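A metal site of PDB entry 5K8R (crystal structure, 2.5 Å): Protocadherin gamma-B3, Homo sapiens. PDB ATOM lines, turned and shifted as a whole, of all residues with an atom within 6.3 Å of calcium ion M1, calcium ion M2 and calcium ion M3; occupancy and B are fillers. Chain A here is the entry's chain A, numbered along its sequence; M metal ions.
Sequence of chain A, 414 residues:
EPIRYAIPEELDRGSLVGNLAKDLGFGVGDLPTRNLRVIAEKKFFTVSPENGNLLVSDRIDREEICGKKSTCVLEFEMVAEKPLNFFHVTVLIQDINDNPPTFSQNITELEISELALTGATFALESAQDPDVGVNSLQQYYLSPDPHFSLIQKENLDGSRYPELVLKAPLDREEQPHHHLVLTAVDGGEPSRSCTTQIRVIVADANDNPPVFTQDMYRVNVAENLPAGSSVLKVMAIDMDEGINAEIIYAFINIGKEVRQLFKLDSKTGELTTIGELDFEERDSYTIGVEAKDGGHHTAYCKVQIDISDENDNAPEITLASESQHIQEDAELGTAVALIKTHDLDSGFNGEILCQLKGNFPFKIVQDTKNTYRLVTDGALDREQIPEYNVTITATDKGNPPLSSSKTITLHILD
N of Asp 186 sits at hydrogen-bond distance from OE1 of Gln 138 (3.5 Å). OD1 of Asp 95 sits close to NE of Arg 62 (3.0 Å). OD1 of Asp 98 lies close to OD1 of Asn 99 (3.4 Å). The side-chain carboxylate (OD2) of Asp 61 sits at hydrogen-bond distance from the backbone NH (N) of Glu 64 (3.3 Å). N of Glu 10 lies within hydrogen-bond range of O of Ile 60 (3.0 Å). The backbone NH (N) of Arg 62 lies close to the side-chain carboxylate (OE1) of Glu 9 (2.8 Å). The side-chain carboxylate of Asp 129 lies close to the side-chain amide nitrogen of Gln 138 (3.0 Å). OE1 of Glu 10 is in salt-bridge range of NE of Arg 59 (2.8 Å).
Within 4 Å of calcium ion M1: Glu 9, Glu 10, Asp 61, Glu 63 and Asp 98. The nearest printed residue that does not touch calcium ion M1 is Asn 99 (4.2 Å).
Of the 27 residues printed, 7 come within 4 Å of calcium ion M2. The nearest printed residue that does not touch calcium ion M2 is Arg 62 (4.5 Å).
Within 4 Å of calcium ion M3: Asn 97, Asn 99, Asp 129, Asp 131, Asn 135 and Asp 186. Along chain A the residues within 4 Å of calcium ion M3 span positions 97 to 186.
OD1 of Asp 61 binds calcium ion M1, 2.4 Å away. OD2 of Asp 98 is bound to calcium ion M1, at 2.4 Å. Calcium ion M1 is bound by the side-chain carboxylate (OE1) of Glu 63 (2.4 Å). OE2 of Glu 10 binds calcium ion M1 (2.6 Å). OE1 of Glu 9 binds calcium ion M1 (2.7 Å). Calcium ion M1 has five donor atoms within binding distance.
Calcium ion M2 is bound by the backbone carbonyl oxygen (O) of Ile 96 (2.4 Å), the side-chain carboxylate (OD1) of Asp 95 (2.4 Å), the side-chain carboxylate (OE2) of Glu 63 (2.4 Å), the side-chain carboxylate (OD1) of Asp 98 (2.5 Å), the side-chain carboxylate (OD1) of Asp 131 (2.5 Å), the side-chain carboxylate (OE2) of Glu 9 (2.5 Å) and the side-chain carboxylate (OE1) of Glu 63 (2.8 Å).
Calcium ion M3 is bound by the backbone carbonyl oxygen (O) of Asn 99 (2.4 Å), the side-chain carboxylate (OD2) of Asp 129 (2.4 Å), the backbone carbonyl oxygen (O) of Asn 135 (2.4 Å), the side-chain amide oxygen (OD1) of Asn 97 (2.4 Å), the side-chain carboxylate (OD2) of Asp 131 (2.5 Å), the side-chain carboxylate (OD1) of Asp 129 (2.7 Å) and the side-chain carboxylate (OD2) of Asp 186 (2.7 Å).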
ATOM      1  N   GLU A   9      -0.363  26.030   4.212  1.00  0.00           N
ATOM      2  CA  GLU A   9      -1.093  27.175   3.705  1.00  0.00           C
ATOM      3  C   GLU A   9      -2.307  26.731   2.900  1.00  0.00           C
ATOM      4  O   GLU A   9      -2.484  25.547   2.573  1.00  0.00           O
ATOM      5  CB  GLU A   9      -0.182  28.053   2.837  1.00  0.00           C
ATOM      6  CG  GLU A   9       0.487  27.283   1.705  1.00  0.00           C
ATOM      7  CD  GLU A   9       1.132  28.197   0.674  1.00  0.00           C
ATOM      8  OE1 GLU A   9       0.654  29.335   0.493  1.00  0.00           O
ATOM      9  OE2 GLU A   9       2.123  27.775   0.048  1.00  0.00           O
ATOM     10  N   GLU A  10      -3.171  27.694   2.587  1.00  0.00           N
ATOM     11  CA  GLU A  10      -4.323  27.497   1.707  1.00  0.00           C
ATOM     12  C   GLU A  10      -5.313  26.471   2.244  1.00  0.00           C
ATOM     13  O   GLU A  10      -5.974  25.763   1.482  1.00  0.00           O
ATOM     14  CB  GLU A  10      -3.872  27.102   0.286  1.00  0.00           C
ATOM     15  CG  GLU A  10      -2.860  28.048  -0.335  1.00  0.00           C
ATOM     16  CD  GLU A  10      -3.473  29.362  -0.784  1.00  0.00           C
ATOM     17  OE1 GLU A  10      -4.716  29.493  -0.735  1.00  0.00           O
ATOM     18  OE2 GLU A  10      -2.711  30.262  -1.193  1.00  0.00           O
ATOM     19  N   ARG A  59      -8.347  33.043   4.056  1.00  0.00           N
ATOM     20  CA  ARG A  59      -7.327  32.420   3.239  1.00  0.00           C
ATOM     21  C   ARG A  59      -5.940  32.817   3.715  1.00  0.00           C
ATOM     22  O   ARG A  59      -5.640  34.010   3.886  1.00  0.00           O
ATOM     23  CB  ARG A  59      -7.509  32.814   1.766  1.00  0.00           C
ATOM     24  CG  ARG A  59      -6.418  32.292   0.858  1.00  0.00           C
ATOM     25  CD  ARG A  59      -6.768  32.497  -0.603  1.00  0.00           C
ATOM     26  NE  ARG A  59      -5.733  31.978  -1.495  1.00  0.00           N
ATOM     27  CZ  ARG A  59      -4.791  32.726  -2.072  1.00  0.00           C
ATOM     28  NH1 ARG A  59      -4.757  34.030  -1.859  1.00  0.00           N
ATOM     29  NH2 ARG A  59      -3.889  32.164  -2.858  1.00  0.00           N
ATOM     30  N   ILE A  60      -5.085  31.826   3.941  1.00  0.00           N
ATOM     31  CA  ILE A  60      -3.716  32.060   4.360  1.00  0.00           C
ATOM     32  C   ILE A  60      -2.777  31.709   3.215  1.00  0.00           C
ATOM     33  O   ILE A  60      -2.383  30.541   3.058  1.00  0.00           O
ATOM     34  CB  ILE A  60      -3.369  31.261   5.637  1.00  0.00           C
ATOM     35  CG1 ILE A  60      -4.337  31.623   6.764  1.00  0.00           C
ATOM     36  CG2 ILE A  60      -1.930  31.520   6.069  1.00  0.00           C
ATOM     37  CD1 ILE A  60      -4.072  30.896   8.057  1.00  0.00           C
ATOM     38  N   ASP A  61      -2.432  32.690   2.394  1.00  0.00           N
ATOM     39  CA  ASP A  61      -1.535  32.502   1.267  1.00  0.00           C
ATOM     40  C   ASP A  61      -0.118  32.846   1.700  1.00  0.00           C
ATOM     41  O   ASP A  61       0.187  34.018   1.970  1.00  0.00           O
ATOM     42  CB  ASP A  61      -1.976  33.358   0.084  1.00  0.00           C
ATOM     43  CG  ASP A  61      -1.005  33.298  -1.080  1.00  0.00           C
ATOM     44  OD1 ASP A  61      -0.331  32.260  -1.245  1.00  0.00           O
ATOM     45  OD2 ASP A  61      -0.914  34.292  -1.839  1.00  0.00           O
ATOM     46  N   ARG A  62       0.749  31.838   1.770  1.00  0.00           N
ATOM     47  CA  ARG A  62       2.116  32.067   2.227  1.00  0.00           C
ATOM     48  C   ARG A  62       2.892  32.967   1.277  1.00  0.00           C
ATOM     49  O   ARG A  62       3.780  33.714   1.711  1.00  0.00           O
ATOM     50  CB  ARG A  62       2.841  30.739   2.408  1.00  0.00           C
ATOM     51  CG  ARG A  62       4.172  30.848   3.136  1.00  0.00           C
ATOM     52  CD  ARG A  62       5.177  29.849   2.599  1.00  0.00           C
ATOM     53  NE  ARG A  62       5.437  30.052   1.180  1.00  0.00           N
ATOM     54  CZ  ARG A  62       6.286  30.960   0.706  1.00  0.00           C
ATOM     55  NH1 ARG A  62       6.965  31.745   1.531  1.00  0.00           N
ATOM     56  NH2 ARG A  62       6.455  31.090  -0.606  1.00  0.00           N
ATOM     57  N   GLU A  63       2.585  32.905  -0.029  1.00  0.00           N
ATOM     58  CA  GLU A  63       3.284  33.751  -0.988  1.00  0.00           C
ATOM     59  C   GLU A  63       2.990  35.230  -0.754  1.00  0.00           C
ATOM     60  O   GLU A  63       3.886  36.072  -0.869  1.00  0.00           O
ATOM     61  CB  GLU A  63       2.907  33.350  -2.413  1.00  0.00           C
ATOM     62  CG  GLU A  63       3.689  32.169  -2.958  1.00  0.00           C
ATOM     63  CD  GLU A  63       3.335  30.863  -2.271  1.00  0.00           C
ATOM     64  OE1 GLU A  63       2.134  30.581  -2.102  1.00  0.00           O
ATOM     65  OE2 GLU A  63       4.266  30.126  -1.888  1.00  0.00           O
ATOM     66  N   GLU A  64       1.748  35.557  -0.418  1.00  0.00           N
ATOM     67  CA  GLU A  64       1.387  36.953  -0.183  1.00  0.00           C
ATOM     68  C   GLU A  64       1.822  37.433   1.199  1.00  0.00           C
ATOM     69  O   GLU A  64       2.072  38.621   1.388  1.00  0.00           O
ATOM     70  CB  GLU A  64      -0.121  37.141  -0.364  1.00  0.00           C
ATOM     71  CG  GLU A  64      -0.573  38.596  -0.345  1.00  0.00           C
ATOM     72  CD  GLU A  64      -2.066  38.724  -0.560  1.00  0.00           C
ATOM     73  OE1 GLU A  64      -2.759  37.682  -0.622  1.00  0.00           O
ATOM     74  OE2 GLU A  64      -2.555  39.877  -0.654  1.00  0.00           O
ATOM     75  N   ASP A  95       4.841  25.736   3.382  1.00  0.00           N
ATOM     76  CA  ASP A  95       4.686  26.035   1.955  1.00  0.00           C
ATOM     77  C   ASP A  95       4.237  24.793   1.201  1.00  0.00           C
ATOM     78  O   ASP A  95       4.747  23.688   1.426  1.00  0.00           O
ATOM     79  CB  ASP A  95       6.012  26.552   1.377  1.00  0.00           C
ATOM     80  CG  ASP A  95       5.896  26.890  -0.103  1.00  0.00           C
ATOM     81  OD1 ASP A  95       4.907  27.561  -0.495  1.00  0.00           O
ATOM     82  OD2 ASP A  95       6.793  26.492  -0.871  1.00  0.00           O
ATOM     83  N   ILE A  96       3.282  24.987   0.286  1.00  0.00           N
ATOM     84  CA  ILE A  96       2.857  23.944  -0.635  1.00  0.00           C
ATOM     85  C   ILE A  96       3.202  24.395  -2.046  1.00  0.00           C
ATOM     86  O   ILE A  96       3.335  25.583  -2.336  1.00  0.00           O
ATOM     87  CB  ILE A  96       1.354  23.617  -0.501  1.00  0.00           C
ATOM     88  CG1 ILE A  96       0.509  24.827  -0.922  1.00  0.00           C
ATOM     89  CG2 ILE A  96       1.026  23.191   0.916  1.00  0.00           C
ATOM     90  CD1 ILE A  96      -0.991  24.583  -0.816  1.00  0.00           C
ATOM     91  N   ASN A  97       3.342  23.416  -2.942  1.00  0.00           N
ATOM     92  CA  ASN A  97       3.708  23.687  -4.334  1.00  0.00           C
ATOM     93  C   ASN A  97       2.432  23.960  -5.129  1.00  0.00           C
ATOM     94  O   ASN A  97       1.956  23.127  -5.913  1.00  0.00           O
ATOM     95  CB  ASN A  97       4.502  22.528  -4.926  1.00  0.00           C
ATOM     96  CG  ASN A  97       5.083  22.858  -6.285  1.00  0.00           C
ATOM     97  OD1 ASN A  97       5.445  23.998  -6.556  1.00  0.00           O
ATOM     98  ND2 ASN A  97       5.157  21.864  -7.155  1.00  0.00           N
ATOM     99  N   ASP A  98       1.864  25.144  -4.926  1.00  0.00           N
ATOM    100  CA  ASP A  98       0.656  25.564  -5.615  1.00  0.00           C
ATOM    101  C   ASP A  98       0.920  26.660  -6.646  1.00  0.00           C
ATOM    102  O   ASP A  98      -0.026  27.293  -7.114  1.00  0.00           O
ATOM    103  CB  ASP A  98      -0.395  26.028  -4.602  1.00  0.00           C
ATOM    104  CG  ASP A  98       0.097  27.155  -3.728  1.00  0.00           C
ATOM    105  OD1 ASP A  98       1.328  27.311  -3.585  1.00  0.00           O
ATOM    106  OD2 ASP A  98      -0.754  27.892  -3.176  1.00  0.00           O
ATOM    107  N   ASN A  99       2.176  26.886  -7.000  1.00  0.00           N
ATOM    108  CA  ASN A  99       2.542  27.891  -7.986  1.00  0.00           C
ATOM    109  C   ASN A  99       3.506  27.269  -8.992  1.00  0.00           C
ATOM    110  O   ASN A  99       4.514  26.664  -8.591  1.00  0.00           O
ATOM    111  CB  ASN A  99       3.185  29.119  -7.332  1.00  0.00           C
ATOM    112  CG  ASN A  99       2.179  29.980  -6.595  1.00  0.00           C
ATOM    113  OD1 ASN A  99       2.244  30.114  -5.374  1.00  0.00           O
ATOM    114  ND2 ASN A  99       1.244  30.564  -7.340  1.00  0.00           N
ATOM    115  N   PRO A 100       3.243  27.388 -10.292  1.00  0.00           N
ATOM    116  CA  PRO A 100       4.161  26.863 -11.283  1.00  0.00           C
ATOM    117  C   PRO A 100       5.292  27.844 -11.545  1.00  0.00           C
ATOM    118  O   PRO A 100       5.161  29.041 -11.255  1.00  0.00           O
ATOM    119  CB  PRO A 100       3.273  26.700 -12.522  1.00  0.00           C
ATOM    120  CG  PRO A 100       2.284  27.808 -12.395  1.00  0.00           C
ATOM    121  CD  PRO A 100       2.029  27.959 -10.911  1.00  0.00           C
ATOM    122  N   PRO A 101       6.420  27.375 -12.089  1.00  0.00           N
ATOM    123  CA  PRO A 101       7.453  28.307 -12.527  1.00  0.00           C
ATOM    124  C   PRO A 101       6.971  29.121 -13.713  1.00  0.00           C
ATOM    125  O   PRO A 101       5.964  28.811 -14.357  1.00  0.00           O
ATOM    126  CB  PRO A 101       8.615  27.387 -12.932  1.00  0.00           C
ATOM    127  CG  PRO A 101       7.966  26.068 -13.234  1.00  0.00           C
ATOM    128  CD  PRO A 101       6.806  25.967 -12.292  1.00  0.00           C
ATOM    129  N   ASP A 129       9.773  31.420  -9.485  1.00  0.00           N
ATOM    130  CA  ASP A 129       8.777  30.632  -8.770  1.00  0.00           C
ATOM    131  C   ASP A 129       8.516  31.271  -7.405  1.00  0.00           C
ATOM    132  O   ASP A 129       9.427  31.351  -6.569  1.00  0.00           O
ATOM    133  CB  ASP A 129       9.250  29.188  -8.606  1.00  0.00           C
ATOM    134  CG  ASP A 129       8.119  28.231  -8.297  1.00  0.00           C
ATOM    135  OD1 ASP A 129       7.295  28.548  -7.412  1.00  0.00           O
ATOM    136  OD2 ASP A 129       8.066  27.157  -8.930  1.00  0.00           O
ATOM    137  N   PRO A 130       7.286  31.737  -7.137  1.00  0.00           N
ATOM    138  CA  PRO A 130       7.015  32.397  -5.860  1.00  0.00           C
ATOM    139  C   PRO A 130       7.030  31.473  -4.662  1.00  0.00           C
ATOM    140  O   PRO A 130       6.946  31.956  -3.521  1.00  0.00           O
ATOM    141  CB  PRO A 130       5.621  33.018  -6.070  1.00  0.00           C
ATOM    142  CG  PRO A 130       5.000  32.156  -7.116  1.00  0.00           C
ATOM    143  CD  PRO A 130       6.107  31.720  -8.023  1.00  0.00           C
ATOM    144  N   ASP A 131       7.120  30.155  -4.873  1.00  0.00           N
ATOM    145  CA  ASP A 131       7.230  29.226  -3.760  1.00  0.00           C
ATOM    146  C   ASP A 131       8.635  29.306  -3.156  1.00  0.00           C
ATOM    147  O   ASP A 131       9.491  30.078  -3.592  1.00  0.00           O
ATOM    148  CB  ASP A 131       6.918  27.804  -4.221  1.00  0.00           C
ATOM    149  CG  ASP A 131       5.479  27.655  -4.704  1.00  0.00           C
ATOM    150  OD1 ASP A 131       4.602  28.368  -4.178  1.00  0.00           O
ATOM    151  OD2 ASP A 131       5.241  26.822  -5.607  1.00  0.00           O
ATOM    152  N   VAL A 132       8.875  28.496  -2.126  1.00  0.00           N
ATOM    153  CA  VAL A 132      10.159  28.437  -1.443  1.00  0.00           C
ATOM    154  C   VAL A 132      10.563  26.991  -1.246  1.00  0.00           C
ATOM    155  O   VAL A 132       9.763  26.062  -1.453  1.00  0.00           O
ATOM    156  CB  VAL A 132      10.128  29.184  -0.085  1.00  0.00           C
ATOM    157  CG1 VAL A 132      10.010  30.687  -0.306  1.00  0.00           C
ATOM    158  CG2 VAL A 132       8.996  28.672   0.773  1.00  0.00           C
ATOM    159  N   VAL A 134      12.079  23.375  -1.846  1.00  0.00           N
ATOM    160  CA  VAL A 134      12.107  22.541  -3.049  1.00  0.00           C
ATOM    161  C   VAL A 134      10.977  22.877  -3.998  1.00  0.00           C
ATOM    162  O   VAL A 134      11.054  22.538  -5.191  1.00  0.00           O
ATOM    163  CB  VAL A 134      12.058  21.051  -2.657  1.00  0.00           C
ATOM    164  CG1 VAL A 134      13.280  20.674  -1.832  1.00  0.00           C
ATOM    165  CG2 VAL A 134      10.783  20.737  -1.903  1.00  0.00           C
ATOM    166  N   ASN A 135       9.924  23.545  -3.511  1.00  0.00           N
ATOM    167  CA  ASN A 135       8.806  23.897  -4.380  1.00  0.00           C
ATOM    168  C   ASN A 135       9.180  24.960  -5.406  1.00  0.00           C
ATOM    169  O   ASN A 135       8.466  25.128  -6.395  1.00  0.00           O
ATOM    170  CB  ASN A 135       7.624  24.377  -3.538  1.00  0.00           C
ATOM    171  CG  ASN A 135       7.144  23.341  -2.560  1.00  0.00           C
ATOM    172  OD1 ASN A 135       7.325  22.135  -2.770  1.00  0.00           O
ATOM    173  ND2 ASN A 135       6.528  23.790  -1.468  1.00  0.00           N
ATOM    174  N   SER A 136      10.293  25.671  -5.197  1.00  0.00           N
ATOM    175  CA  SER A 136      10.791  26.634  -6.170  1.00  0.00           C
ATOM    176  C   SER A 136      12.130  26.221  -6.781  1.00  0.00           C
ATOM    177  O   SER A 136      12.598  26.904  -7.697  1.00  0.00           O
ATOM    178  CB  SER A 136      10.938  28.021  -5.539  1.00  0.00           C
ATOM    179  OG  SER A 136      11.848  27.987  -4.455  1.00  0.00           O
ATOM    180  N   GLN A 138      14.306  24.718  -9.288  1.00  0.00           N
ATOM    181  CA  GLN A 138      13.977  24.436 -10.669  1.00  0.00           C
ATOM    182  C   GLN A 138      14.943  23.437 -11.296  1.00  0.00           C
ATOM    183  O   GLN A 138      16.090  23.284 -10.860  1.00  0.00           O
ATOM    184  CB  GLN A 138      13.966  25.727 -11.498  1.00  0.00           C
ATOM    185  CG  GLN A 138      12.978  26.764 -11.008  1.00  0.00           C
ATOM    186  CD  GLN A 138      11.557  26.232 -10.931  1.00  0.00           C
ATOM    187  OE1 GLN A 138      11.127  25.450 -11.787  1.00  0.00           O
ATOM    188  NE2 GLN A 138      10.835  26.631  -9.897  1.00  0.00           N
ATOM    189  N   ASP A 186       9.684  22.335 -11.396  1.00  0.00           N
ATOM    190  CA  ASP A 186      10.061  22.516 -10.007  1.00  0.00           C
ATOM    191  C   ASP A 186      10.155  21.168  -9.290  1.00  0.00           C
ATOM    192  O   ASP A 186       9.858  20.115  -9.858  1.00  0.00           O
ATOM    193  CB  ASP A 186       9.071  23.456  -9.299  1.00  0.00           C
ATOM    194  CG  ASP A 186       7.629  23.008  -9.426  1.00  0.00           C
ATOM    195  OD1 ASP A 186       7.364  21.786  -9.560  1.00  0.00           O
ATOM    196  OD2 ASP A 186       6.738  23.879  -9.380  1.00  0.00           O
ATOM    197  N   GLY A 187      10.579  21.200  -8.030  1.00  0.00           N
ATOM    198  CA  GLY A 187      10.753  19.980  -7.272  1.00  0.00           C
ATOM    199  C   GLY A 187       9.699  19.773  -6.200  1.00  0.00           C
ATOM    200  O   GLY A 187       9.945  19.095  -5.210  1.00  0.00           O
ATOM    201  N   GLY A 188       8.520  20.375  -6.387  1.00  0.00           N
ATOM    202  CA  GLY A 188       7.449  20.263  -5.434  1.00  0.00           C
ATOM    203  C   GLY A 188       6.509  19.113  -5.747  1.00  0.00           C
ATOM    204  O   GLY A 188       6.706  18.327  -6.669  1.00  0.00           O
ATOM    205  N   ARG A 192       5.276  20.942 -11.088  1.00  0.00           N
ATOM    206  CA  ARG A 192       4.738  21.963 -11.986  1.00  0.00           C
ATOM    207  C   ARG A 192       5.848  22.459 -12.899  1.00  0.00           C
ATOM    208  O   ARG A 192       7.010  22.560 -12.481  1.00  0.00           O
ATOM    209  CB  ARG A 192       4.139  23.132 -11.196  1.00  0.00           C
ATOM    210  CG  ARG A 192       2.838  22.778 -10.483  1.00  0.00           C
ATOM    211  CD  ARG A 192       2.320  23.949  -9.661  1.00  0.00           C
ATOM    212  NE  ARG A 192       0.861  24.005  -9.660  1.00  0.00           N
ATOM    213  CZ  ARG A 192       0.084  23.294  -8.842  1.00  0.00           C
ATOM    214  NH1 ARG A 192       0.630  22.474  -7.959  1.00  0.00           N
ATOM    215  NH2 ARG A 192      -1.235  23.417  -8.914  1.00  0.00           N
HETATM  216 CA    CA M   1      -0.228  29.963  -1.992  1.00  0.00          CA
HETATM  217 CA    CA M   2       3.227  27.971  -2.166  1.00  0.00          CA
HETATM  218 CA    CA M   3       6.529  25.929  -7.572  1.00  0.00          CA
